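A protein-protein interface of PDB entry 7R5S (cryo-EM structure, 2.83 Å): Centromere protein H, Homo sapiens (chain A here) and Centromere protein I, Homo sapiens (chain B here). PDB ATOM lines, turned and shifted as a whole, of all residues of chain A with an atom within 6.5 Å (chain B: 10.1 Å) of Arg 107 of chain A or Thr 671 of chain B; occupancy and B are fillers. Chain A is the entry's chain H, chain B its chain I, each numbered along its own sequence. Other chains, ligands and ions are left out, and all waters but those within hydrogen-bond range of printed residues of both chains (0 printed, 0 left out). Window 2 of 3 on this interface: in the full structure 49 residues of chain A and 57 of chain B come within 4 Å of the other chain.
Leu 103 of chain A touches none of the printed residues of chain B. No residue of chain B comes within 4 Å of Asp 104 of chain A. Printed residues of chain B within 4 Å of Arg 105 of chain A: Leu 593. Arg 107 of chain A touches just one residue of chain B: Thr 671 (3.6 Å). Thr 110 of chain A touches just one residue of chain B: Val 673. No residue of chain B comes within 4 Å of Ala 111 of chain A. Leu 112 of chain A touches none of the printed residues of chain B. Thr 671 of chain B touches one residue of chain A. Printed residues of chain A within 4 Å of His 684 of chain B: Ser 109 (3.0 Å). Printed residues of chain A within 4 Å of Pro 686 of chain B: Ser 109. The nearest residue of chain A that does not touch Thr 671 of chain B is Leu 103 of chain A (5.2 Å). The nearest printed residue of chain A that does not touch Leu 593 of chain B is Leu 103 of chain A (6.1 Å).
Of the 11 printed residues of chain A, 6 touch a printed residue of chain B. Hydrophobic or aromatic side chains of chain A within 4 Å of the printed part of chain B: Ala 102 and Met 106. Of the 20 printed residues of chain B, 7 touch a printed residue of chain A. Along chain B the printed residues that touch a printed residue of chain A span positions 593 to 686. Among the printed residues, 8 pairs touch across the chains.
Among the printed residues, pairs that only touch across the chains: Ala 102 of chain A with Leu 593 of chain B (3.7 Å), Met 106 of chain A with Phe 657 of chain B (3.6 Å), Arg 107 of chain A with Thr 671 of chain B (3.6 Å), Ser 109 of chain A with Pro 686 of chain B (3.99 Å) and Thr 110 of chain A with Val 673 of chain B (3.9 Å).
O of Leu 593 of chain B is in hydrogen-bond range of NE of Arg 105 of chain A. OG of Ser 109 of chain A sits at hydrogen-bond distance from O of His 684 of chain B (3.0 Å). O of Ser 679 of chain B is in hydrogen-bond range of OG of Ser 109 of chain A.
The backbone carbonyl oxygen (O) of Leu 668 of chain B sits at hydrogen-bond distance from the backbone NH (N) of Val 673 of chain B (2.8 Å). OD2 of Asp 104 of chain A is in salt-bridge range of NH2 of Arg 107 of chain A, 3.2 Å away. The backbone carbonyl oxygen (O) of Ile 667 of chain B lies within hydrogen-bond range of the side-chain hydroxyl (OG1) of Thr 671 of chain B, 2.7 Å away. The side-chain hydroxyl of Ser 679 of chain B is in hydrogen-bond range of the backbone carbonyl oxygen of Tyr 676 of chain B (2.8 Å).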
ATOM      1  N   ALA A 102     -36.955  24.960 -31.346  1.00  0.00           N
ATOM      2  CA  ALA A 102     -35.496  25.011 -31.351  1.00  0.00           C
ATOM      3  C   ALA A 102     -34.957  25.549 -30.032  1.00  0.00           C
ATOM      4  O   ALA A 102     -33.982  25.015 -29.486  1.00  0.00           O
ATOM      5  CB  ALA A 102     -35.004  25.862 -32.521  1.00  0.00           C
ATOM      6  N   LEU A 103     -35.579  26.605 -29.503  1.00  0.00           N
ATOM      7  CA  LEU A 103     -35.129  27.159 -28.229  1.00  0.00           C
ATOM      8  C   LEU A 103     -35.278  26.140 -27.104  1.00  0.00           C
ATOM      9  O   LEU A 103     -34.365  25.959 -26.284  1.00  0.00           O
ATOM     10  CB  LEU A 103     -35.904  28.436 -27.909  1.00  0.00           C
ATOM     11  CG  LEU A 103     -35.533  29.136 -26.600  1.00  0.00           C
ATOM     12  CD1 LEU A 103     -34.063  29.523 -26.597  1.00  0.00           C
ATOM     13  CD2 LEU A 103     -36.412  30.356 -26.377  1.00  0.00           C
ATOM     14  N   ASP A 104     -36.428  25.459 -27.052  1.00  0.00           N
ATOM     15  CA  ASP A 104     -36.640  24.460 -26.009  1.00  0.00           C
ATOM     16  C   ASP A 104     -35.643  23.313 -26.128  1.00  0.00           C
ATOM     17  O   ASP A 104     -35.130  22.821 -25.113  1.00  0.00           O
ATOM     18  CB  ASP A 104     -38.073  23.937 -26.066  1.00  0.00           C
ATOM     19  CG  ASP A 104     -39.070  24.898 -25.447  1.00  0.00           C
ATOM     20  OD1 ASP A 104     -40.288  24.698 -25.634  1.00  0.00           O
ATOM     21  OD2 ASP A 104     -38.634  25.856 -24.774  1.00  0.00           O
ATOM     22  N   ARG A 105     -35.347  22.881 -27.356  1.00  0.00           N
ATOM     23  CA  ARG A 105     -34.400  21.787 -27.542  1.00  0.00           C
ATOM     24  C   ARG A 105     -32.997  22.193 -27.117  1.00  0.00           C
ATOM     25  O   ARG A 105     -32.281  21.405 -26.490  1.00  0.00           O
ATOM     26  CB  ARG A 105     -34.406  21.322 -28.999  1.00  0.00           C
ATOM     27  CG  ARG A 105     -35.626  20.504 -29.382  1.00  0.00           C
ATOM     28  CD  ARG A 105     -35.859  19.369 -28.401  1.00  0.00           C
ATOM     29  NE  ARG A 105     -37.083  18.632 -28.704  1.00  0.00           N
ATOM     30  CZ  ARG A 105     -37.600  17.690 -27.924  1.00  0.00           C
ATOM     31  NH1 ARG A 105     -37.002  17.367 -26.785  1.00  0.00           N
ATOM     32  NH2 ARG A 105     -38.717  17.071 -28.279  1.00  0.00           N
ATOM     33  N   MET A 106     -32.585  23.423 -27.440  1.00  0.00           N
ATOM     34  CA  MET A 106     -31.264  23.882 -27.017  1.00  0.00           C
ATOM     35  C   MET A 106     -31.173  23.975 -25.498  1.00  0.00           C
ATOM     36  O   MET A 106     -30.154  23.594 -24.902  1.00  0.00           O
ATOM     37  CB  MET A 106     -30.945  25.232 -27.659  1.00  0.00           C
ATOM     38  CG  MET A 106     -30.619  25.151 -29.140  1.00  0.00           C
ATOM     39  SD  MET A 106     -30.053  26.724 -29.815  1.00  0.00           S
ATOM     40  CE  MET A 106     -29.668  26.246 -31.497  1.00  0.00           C
ATOM     41  N   ARG A 107     -32.230  24.481 -24.853  1.00  0.00           N
ATOM     42  CA  ARG A 107     -32.239  24.553 -23.396  1.00  0.00           C
ATOM     43  C   ARG A 107     -32.130  23.165 -22.775  1.00  0.00           C
ATOM     44  O   ARG A 107     -31.337  22.943 -21.850  1.00  0.00           O
ATOM     45  CB  ARG A 107     -33.507  25.260 -22.913  1.00  0.00           C
ATOM     46  CG  ARG A 107     -33.340  26.752 -22.685  1.00  0.00           C
ATOM     47  CD  ARG A 107     -34.197  27.227 -21.525  1.00  0.00           C
ATOM     48  NE  ARG A 107     -35.622  27.076 -21.800  1.00  0.00           N
ATOM     49  CZ  ARG A 107     -36.406  28.054 -22.244  1.00  0.00           C
ATOM     50  NH1 ARG A 107     -35.901  29.260 -22.466  1.00  0.00           N
ATOM     51  NH2 ARG A 107     -37.692  27.825 -22.468  1.00  0.00           N
ATOM     52  N   LEU A 108     -32.925  22.214 -23.274  1.00  0.00           N
ATOM     53  CA  LEU A 108     -32.853  20.852 -22.758  1.00  0.00           C
ATOM     54  C   LEU A 108     -31.472  20.249 -22.985  1.00  0.00           C
ATOM     55  O   LEU A 108     -30.939  19.556 -22.112  1.00  0.00           O
ATOM     56  CB  LEU A 108     -33.929  19.982 -23.406  1.00  0.00           C
ATOM     57  CG  LEU A 108     -33.918  18.504 -23.011  1.00  0.00           C
ATOM     58  CD1 LEU A 108     -34.054  18.348 -21.505  1.00  0.00           C
ATOM     59  CD2 LEU A 108     -35.018  17.743 -23.733  1.00  0.00           C
ATOM     60  N   SER A 109     -30.869  20.521 -24.144  1.00  0.00           N
ATOM     61  CA  SER A 109     -29.565  19.948 -24.457  1.00  0.00           C
ATOM     62  C   SER A 109     -28.495  20.460 -23.503  1.00  0.00           C
ATOM     63  O   SER A 109     -27.697  19.677 -22.974  1.00  0.00           O
ATOM     64  CB  SER A 109     -29.189  20.262 -25.906  1.00  0.00           C
ATOM     65  OG  SER A 109     -27.826  19.964 -26.153  1.00  0.00           O
ATOM     66  N   THR A 110     -28.462  21.774 -23.262  1.00  0.00           N
ATOM     67  CA  THR A 110     -27.439  22.300 -22.361  1.00  0.00           C
ATOM     68  C   THR A 110     -27.691  21.861 -20.921  1.00  0.00           C
ATOM     69  O   THR A 110     -26.744  21.524 -20.196  1.00  0.00           O
ATOM     70  CB  THR A 110     -27.348  23.827 -22.466  1.00  0.00           C
ATOM     71  OG1 THR A 110     -26.377  24.313 -21.530  1.00  0.00           O
ATOM     72  CG2 THR A 110     -28.684  24.490 -22.185  1.00  0.00           C
ATOM     73  N   ALA A 111     -28.961  21.820 -20.494  1.00  0.00           N
ATOM     74  CA  ALA A 111     -29.259  21.381 -19.136  1.00  0.00           C
ATOM     75  C   ALA A 111     -28.924  19.910 -18.931  1.00  0.00           C
ATOM     76  O   ALA A 111     -28.557  19.507 -17.822  1.00  0.00           O
ATOM     77  CB  ALA A 111     -30.729  21.641 -18.808  1.00  0.00           C
ATOM     78  N   LEU A 112     -29.041  19.096 -19.982  1.00  0.00           N
ATOM     79  CA  LEU A 112     -28.692  17.686 -19.880  1.00  0.00           C
ATOM     80  C   LEU A 112     -27.187  17.467 -19.951  1.00  0.00           C
ATOM     81  O   LEU A 112     -26.665  16.559 -19.296  1.00  0.00           O
ATOM     82  CB  LEU A 112     -29.394  16.899 -20.988  1.00  0.00           C
ATOM     83  CG  LEU A 112     -29.536  15.389 -20.821  1.00  0.00           C
ATOM     84  CD1 LEU A 112     -30.326  15.062 -19.567  1.00  0.00           C
ATOM     85  CD2 LEU A 112     -30.211  14.803 -22.046  1.00  0.00           C
ATOM     86  N   LEU B 593     -35.375  18.136 -35.127  1.00  0.00           N
ATOM     87  CA  LEU B 593     -35.303  18.432 -33.701  1.00  0.00           C
ATOM     88  C   LEU B 593     -36.069  17.420 -32.856  1.00  0.00           C
ATOM     89  O   LEU B 593     -36.593  17.769 -31.793  1.00  0.00           O
ATOM     90  CB  LEU B 593     -35.818  19.845 -33.433  1.00  0.00           C
ATOM     91  CG  LEU B 593     -35.022  20.986 -34.069  1.00  0.00           C
ATOM     92  CD1 LEU B 593     -35.743  22.309 -33.887  1.00  0.00           C
ATOM     93  CD2 LEU B 593     -33.621  21.052 -33.483  1.00  0.00           C
ATOM     94  N   PHE B 657     -27.111  28.360 -36.475  1.00  0.00           N
ATOM     95  CA  PHE B 657     -27.975  29.510 -36.745  1.00  0.00           C
ATOM     96  C   PHE B 657     -27.954  29.812 -38.241  1.00  0.00           C
ATOM     97  O   PHE B 657     -27.275  30.722 -38.722  1.00  0.00           O
ATOM     98  CB  PHE B 657     -27.541  30.711 -35.915  1.00  0.00           C
ATOM     99  CG  PHE B 657     -27.928  30.611 -34.469  1.00  0.00           C
ATOM    100  CD1 PHE B 657     -28.890  29.702 -34.061  1.00  0.00           C
ATOM    101  CD2 PHE B 657     -27.331  31.420 -33.519  1.00  0.00           C
ATOM    102  CE1 PHE B 657     -29.251  29.603 -32.732  1.00  0.00           C
ATOM    103  CE2 PHE B 657     -27.687  31.325 -32.188  1.00  0.00           C
ATOM    104  CZ  PHE B 657     -28.650  30.415 -31.795  1.00  0.00           C
ATOM    105  N   ILE B 663     -32.395  32.657 -34.281  1.00  0.00           N
ATOM    106  CA  ILE B 663     -32.467  33.068 -32.884  1.00  0.00           C
ATOM    107  C   ILE B 663     -31.202  33.851 -32.562  1.00  0.00           C
ATOM    108  O   ILE B 663     -30.093  33.304 -32.615  1.00  0.00           O
ATOM    109  CB  ILE B 663     -32.630  31.866 -31.942  1.00  0.00           C
ATOM    110  CG1 ILE B 663     -33.961  31.158 -32.207  1.00  0.00           C
ATOM    111  CG2 ILE B 663     -32.536  32.309 -30.490  1.00  0.00           C
ATOM    112  CD1 ILE B 663     -34.206  29.963 -31.312  1.00  0.00           C
ATOM    113  N   ASP B 664     -31.367  35.126 -32.229  1.00  0.00           N
ATOM    114  CA  ASP B 664     -30.238  35.981 -31.914  1.00  0.00           C
ATOM    115  C   ASP B 664     -29.719  35.678 -30.509  1.00  0.00           C
ATOM    116  O   ASP B 664     -30.465  35.202 -29.650  1.00  0.00           O
ATOM    117  CB  ASP B 664     -30.646  37.445 -32.044  1.00  0.00           C
ATOM    118  CG  ASP B 664     -30.947  37.840 -33.477  1.00  0.00           C
ATOM    119  OD1 ASP B 664     -30.955  39.054 -33.773  1.00  0.00           O
ATOM    120  OD2 ASP B 664     -31.178  36.936 -34.308  1.00  0.00           O
ATOM    121  N   PRO B 665     -28.434  35.943 -30.247  1.00  0.00           N
ATOM    122  CA  PRO B 665     -27.807  35.412 -29.026  1.00  0.00           C
ATOM    123  C   PRO B 665     -28.201  36.118 -27.736  1.00  0.00           C
ATOM    124  O   PRO B 665     -27.782  35.658 -26.664  1.00  0.00           O
ATOM    125  CB  PRO B 665     -26.308  35.581 -29.303  1.00  0.00           C
ATOM    126  CG  PRO B 665     -26.237  36.734 -30.237  1.00  0.00           C
ATOM    127  CD  PRO B 665     -27.456  36.634 -31.110  1.00  0.00           C
ATOM    128  N   GLU B 666     -28.974  37.206 -27.776  1.00  0.00           N
ATOM    129  CA  GLU B 666     -29.321  37.870 -26.522  1.00  0.00           C
ATOM    130  C   GLU B 666     -30.252  37.005 -25.681  1.00  0.00           C
ATOM    131  O   GLU B 666     -30.165  37.007 -24.447  1.00  0.00           O
ATOM    132  CB  GLU B 666     -29.934  39.252 -26.773  1.00  0.00           C
ATOM    133  CG  GLU B 666     -31.251  39.288 -27.535  1.00  0.00           C
ATOM    134  CD  GLU B 666     -31.075  39.123 -29.028  1.00  0.00           C
ATOM    135  OE1 GLU B 666     -32.083  38.852 -29.714  1.00  0.00           O
ATOM    136  OE2 GLU B 666     -29.934  39.270 -29.515  1.00  0.00           O
ATOM    137  N   ILE B 667     -31.143  36.246 -26.326  1.00  0.00           N
ATOM    138  CA  ILE B 667     -31.987  35.321 -25.575  1.00  0.00           C
ATOM    139  C   ILE B 667     -31.143  34.212 -24.967  1.00  0.00           C
ATOM    140  O   ILE B 667     -31.356  33.820 -23.812  1.00  0.00           O
ATOM    141  CB  ILE B 667     -33.116  34.745 -26.452  1.00  0.00           C
ATOM    142  CG1 ILE B 667     -33.929  35.855 -27.126  1.00  0.00           C
ATOM    143  CG2 ILE B 667     -34.034  33.858 -25.622  1.00  0.00           C
ATOM    144  CD1 ILE B 667     -33.416  36.267 -28.489  1.00  0.00           C
ATOM    145  N   LEU B 668     -30.168  33.697 -25.720  1.00  0.00           N
ATOM    146  CA  LEU B 668     -29.271  32.681 -25.181  1.00  0.00           C
ATOM    147  C   LEU B 668     -28.494  33.215 -23.985  1.00  0.00           C
ATOM    148  O   LEU B 668     -28.217  32.476 -23.034  1.00  0.00           O
ATOM    149  CB  LEU B 668     -28.307  32.200 -26.266  1.00  0.00           C
ATOM    150  CG  LEU B 668     -28.856  32.036 -27.682  1.00  0.00           C
ATOM    151  CD1 LEU B 668     -27.749  31.577 -28.611  1.00  0.00           C
ATOM    152  CD2 LEU B 668     -30.018  31.055 -27.702  1.00  0.00           C
ATOM    153  N   GLU B 669     -28.135  34.500 -24.017  1.00  0.00           N
ATOM    154  CA  GLU B 669     -27.336  35.068 -22.939  1.00  0.00           C
ATOM    155  C   GLU B 669     -28.167  35.374 -21.699  1.00  0.00           C
ATOM    156  O   GLU B 669     -27.692  35.153 -20.579  1.00  0.00           O
ATOM    157  CB  GLU B 669     -26.622  36.332 -23.424  1.00  0.00           C
ATOM    158  CG  GLU B 669     -25.358  36.059 -24.232  1.00  0.00           C
ATOM    159  CD  GLU B 669     -24.519  34.926 -23.660  1.00  0.00           C
ATOM    160  OE1 GLU B 669     -24.268  34.921 -22.435  1.00  0.00           O
ATOM    161  OE2 GLU B 669     -24.115  34.034 -24.435  1.00  0.00           O
ATOM    162  N   LYS B 670     -29.397  35.869 -21.860  1.00  0.00           N
ATOM    163  CA  LYS B 670     -30.225  36.088 -20.677  1.00  0.00           C
ATOM    164  C   LYS B 670     -30.703  34.763 -20.098  1.00  0.00           C
ATOM    165  O   LYS B 670     -30.929  34.653 -18.888  1.00  0.00           O
ATOM    166  CB  LYS B 670     -31.416  36.998 -20.989  1.00  0.00           C
ATOM    167  CG  LYS B 670     -32.245  36.615 -22.198  1.00  0.00           C
ATOM    168  CD  LYS B 670     -33.504  37.474 -22.271  1.00  0.00           C
ATOM    169  CE  LYS B 670     -33.959  37.695 -23.703  1.00  0.00           C
ATOM    170  NZ  LYS B 670     -32.996  38.539 -24.461  1.00  0.00           N
ATOM    171  N   THR B 671     -30.854  33.742 -20.946  1.00  0.00           N
ATOM    172  CA  THR B 671     -31.249  32.429 -20.450  1.00  0.00           C
ATOM    173  C   THR B 671     -30.111  31.761 -19.686  1.00  0.00           C
ATOM    174  O   THR B 671     -30.325  31.208 -18.601  1.00  0.00           O
ATOM    175  CB  THR B 671     -31.709  31.546 -21.610  1.00  0.00           C
ATOM    176  OG1 THR B 671     -32.850  32.141 -22.241  1.00  0.00           O
ATOM    177  CG2 THR B 671     -32.077  30.159 -21.112  1.00  0.00           C
ATOM    178  N   GLY B 672     -28.899  31.805 -20.232  1.00  0.00           N
ATOM    179  CA  GLY B 672     -27.751  31.219 -19.567  1.00  0.00           C
ATOM    180  C   GLY B 672     -27.053  30.156 -20.390  1.00  0.00           C
ATOM    181  O   GLY B 672     -26.346  29.303 -19.843  1.00  0.00           O
ATOM    182  N   VAL B 673     -27.244  30.196 -21.704  1.00  0.00           N
ATOM    183  CA  VAL B 673     -26.614  29.246 -22.615  1.00  0.00           C
ATOM    184  C   VAL B 673     -25.305  29.860 -23.097  1.00  0.00           C
ATOM    185  O   VAL B 673     -25.305  30.791 -23.906  1.00  0.00           O
ATOM    186  CB  VAL B 673     -27.536  28.900 -23.790  1.00  0.00           C
ATOM    187  CG1 VAL B 673     -26.827  27.975 -24.767  1.00  0.00           C
ATOM    188  CG2 VAL B 673     -28.824  28.267 -23.284  1.00  0.00           C
ATOM    189  N   ALA B 674     -24.185  29.338 -22.598  1.00  0.00           N
ATOM    190  CA  ALA B 674     -22.873  29.866 -22.954  1.00  0.00           C
ATOM    191  C   ALA B 674     -22.262  29.153 -24.154  1.00  0.00           C
ATOM    192  O   ALA B 674     -21.694  29.805 -25.037  1.00  0.00           O
ATOM    193  CB  ALA B 674     -21.926  29.773 -21.755  1.00  0.00           C
ATOM    194  N   GLU B 675     -22.364  27.829 -24.204  1.00  0.00           N
ATOM    195  CA  GLU B 675     -21.817  27.024 -25.296  1.00  0.00           C
ATOM    196  C   GLU B 675     -22.988  26.512 -26.132  1.00  0.00           C
ATOM    197  O   GLU B 675     -23.517  25.426 -25.891  1.00  0.00           O
ATOM    198  CB  GLU B 675     -20.964  25.877 -24.760  1.00  0.00           C
ATOM    199  CG  GLU B 675     -20.000  26.279 -23.655  1.00  0.00           C
ATOM    200  CD  GLU B 675     -19.188  27.511 -24.010  1.00  0.00           C
ATOM    201  OE1 GLU B 675     -18.458  27.470 -25.023  1.00  0.00           O
ATOM    202  OE2 GLU B 675     -19.278  28.517 -23.276  1.00  0.00           O
ATOM    203  N   TYR B 676     -23.389  27.309 -27.123  1.00  0.00           N
ATOM    204  CA  TYR B 676     -24.487  26.948 -28.009  1.00  0.00           C
ATOM    205  C   TYR B 676     -24.027  26.492 -29.385  1.00  0.00           C
ATOM    206  O   TYR B 676     -24.843  25.966 -30.149  1.00  0.00           O
ATOM    207  CB  TYR B 676     -25.451  28.131 -28.172  1.00  0.00           C
ATOM    208  CG  TYR B 676     -24.860  29.310 -28.913  1.00  0.00           C
ATOM    209  CD1 TYR B 676     -25.092  29.491 -30.271  1.00  0.00           C
ATOM    210  CD2 TYR B 676     -24.069  30.244 -28.255  1.00  0.00           C
ATOM    211  CE1 TYR B 676     -24.553  30.566 -30.951  1.00  0.00           C
ATOM    212  CE2 TYR B 676     -23.526  31.322 -28.928  1.00  0.00           C
ATOM    213  CZ  TYR B 676     -23.773  31.478 -30.275  1.00  0.00           C
ATOM    214  OH  TYR B 676     -23.235  32.550 -30.950  1.00  0.00           O
ATOM    215  N   SER B 679     -24.174  22.581 -29.295  1.00  0.00           N
ATOM    216  CA  SER B 679     -25.208  22.080 -28.399  1.00  0.00           C
ATOM    217  C   SER B 679     -26.017  20.953 -29.026  1.00  0.00           C
ATOM    218  O   SER B 679     -26.475  20.054 -28.311  1.00  0.00           O
ATOM    219  CB  SER B 679     -26.138  23.220 -27.980  1.00  0.00           C
ATOM    220  OG  SER B 679     -26.494  24.021 -29.093  1.00  0.00           O
ATOM    221  N   LEU B 680     -26.205  20.980 -30.345  1.00  0.00           N
ATOM    222  CA  LEU B 680     -26.989  19.974 -31.051  1.00  0.00           C
ATOM    223  C   LEU B 680     -26.129  19.121 -31.979  1.00  0.00           C
ATOM    224  O   LEU B 680     -26.600  18.666 -33.023  1.00  0.00           O
ATOM    225  CB  LEU B 680     -28.120  20.635 -31.837  1.00  0.00           C
ATOM    226  CG  LEU B 680     -29.190  21.360 -31.019  1.00  0.00           C
ATOM    227  CD1 LEU B 680     -30.185  22.052 -31.934  1.00  0.00           C
ATOM    228  CD2 LEU B 680     -29.900  20.389 -30.090  1.00  0.00           C
ATOM    229  N   HIS B 684     -23.832  15.841 -28.168  1.00  0.00           N
ATOM    230  CA  HIS B 684     -24.674  16.478 -27.166  1.00  0.00           C
ATOM    231  C   HIS B 684     -26.138  16.577 -27.576  1.00  0.00           C
ATOM    232  O   HIS B 684     -26.925  17.198 -26.854  1.00  0.00           O
ATOM    233  CB  HIS B 684     -24.136  17.875 -26.841  1.00  0.00           C
ATOM    234  CG  HIS B 684     -22.716  17.878 -26.368  1.00  0.00           C
ATOM    235  ND1 HIS B 684     -21.893  18.977 -26.491  1.00  0.00           N
ATOM    236  CD2 HIS B 684     -21.973  16.915 -25.773  1.00  0.00           C
ATOM    237  CE1 HIS B 684     -20.704  18.691 -25.992  1.00  0.00           C
ATOM    238  NE2 HIS B 684     -20.725  17.446 -25.550  1.00  0.00           N
ATOM    239  N   PRO B 686     -29.921  15.620 -27.720  1.00  0.00           N
ATOM    240  CA  PRO B 686     -30.745  14.822 -26.798  1.00  0.00           C
ATOM    241  C   PRO B 686     -31.201  13.491 -27.373  1.00  0.00           C
ATOM    242  O   PRO B 686     -31.659  12.634 -26.606  1.00  0.00           O
ATOM    243  CB  PRO B 686     -31.940  15.740 -26.508  1.00  0.00           C
ATOM    244  CG  PRO B 686     -31.455  17.116 -26.831  1.00  0.00           C
ATOM    245  CD  PRO B 686     -30.502  16.948 -27.974  1.00  0.00           C
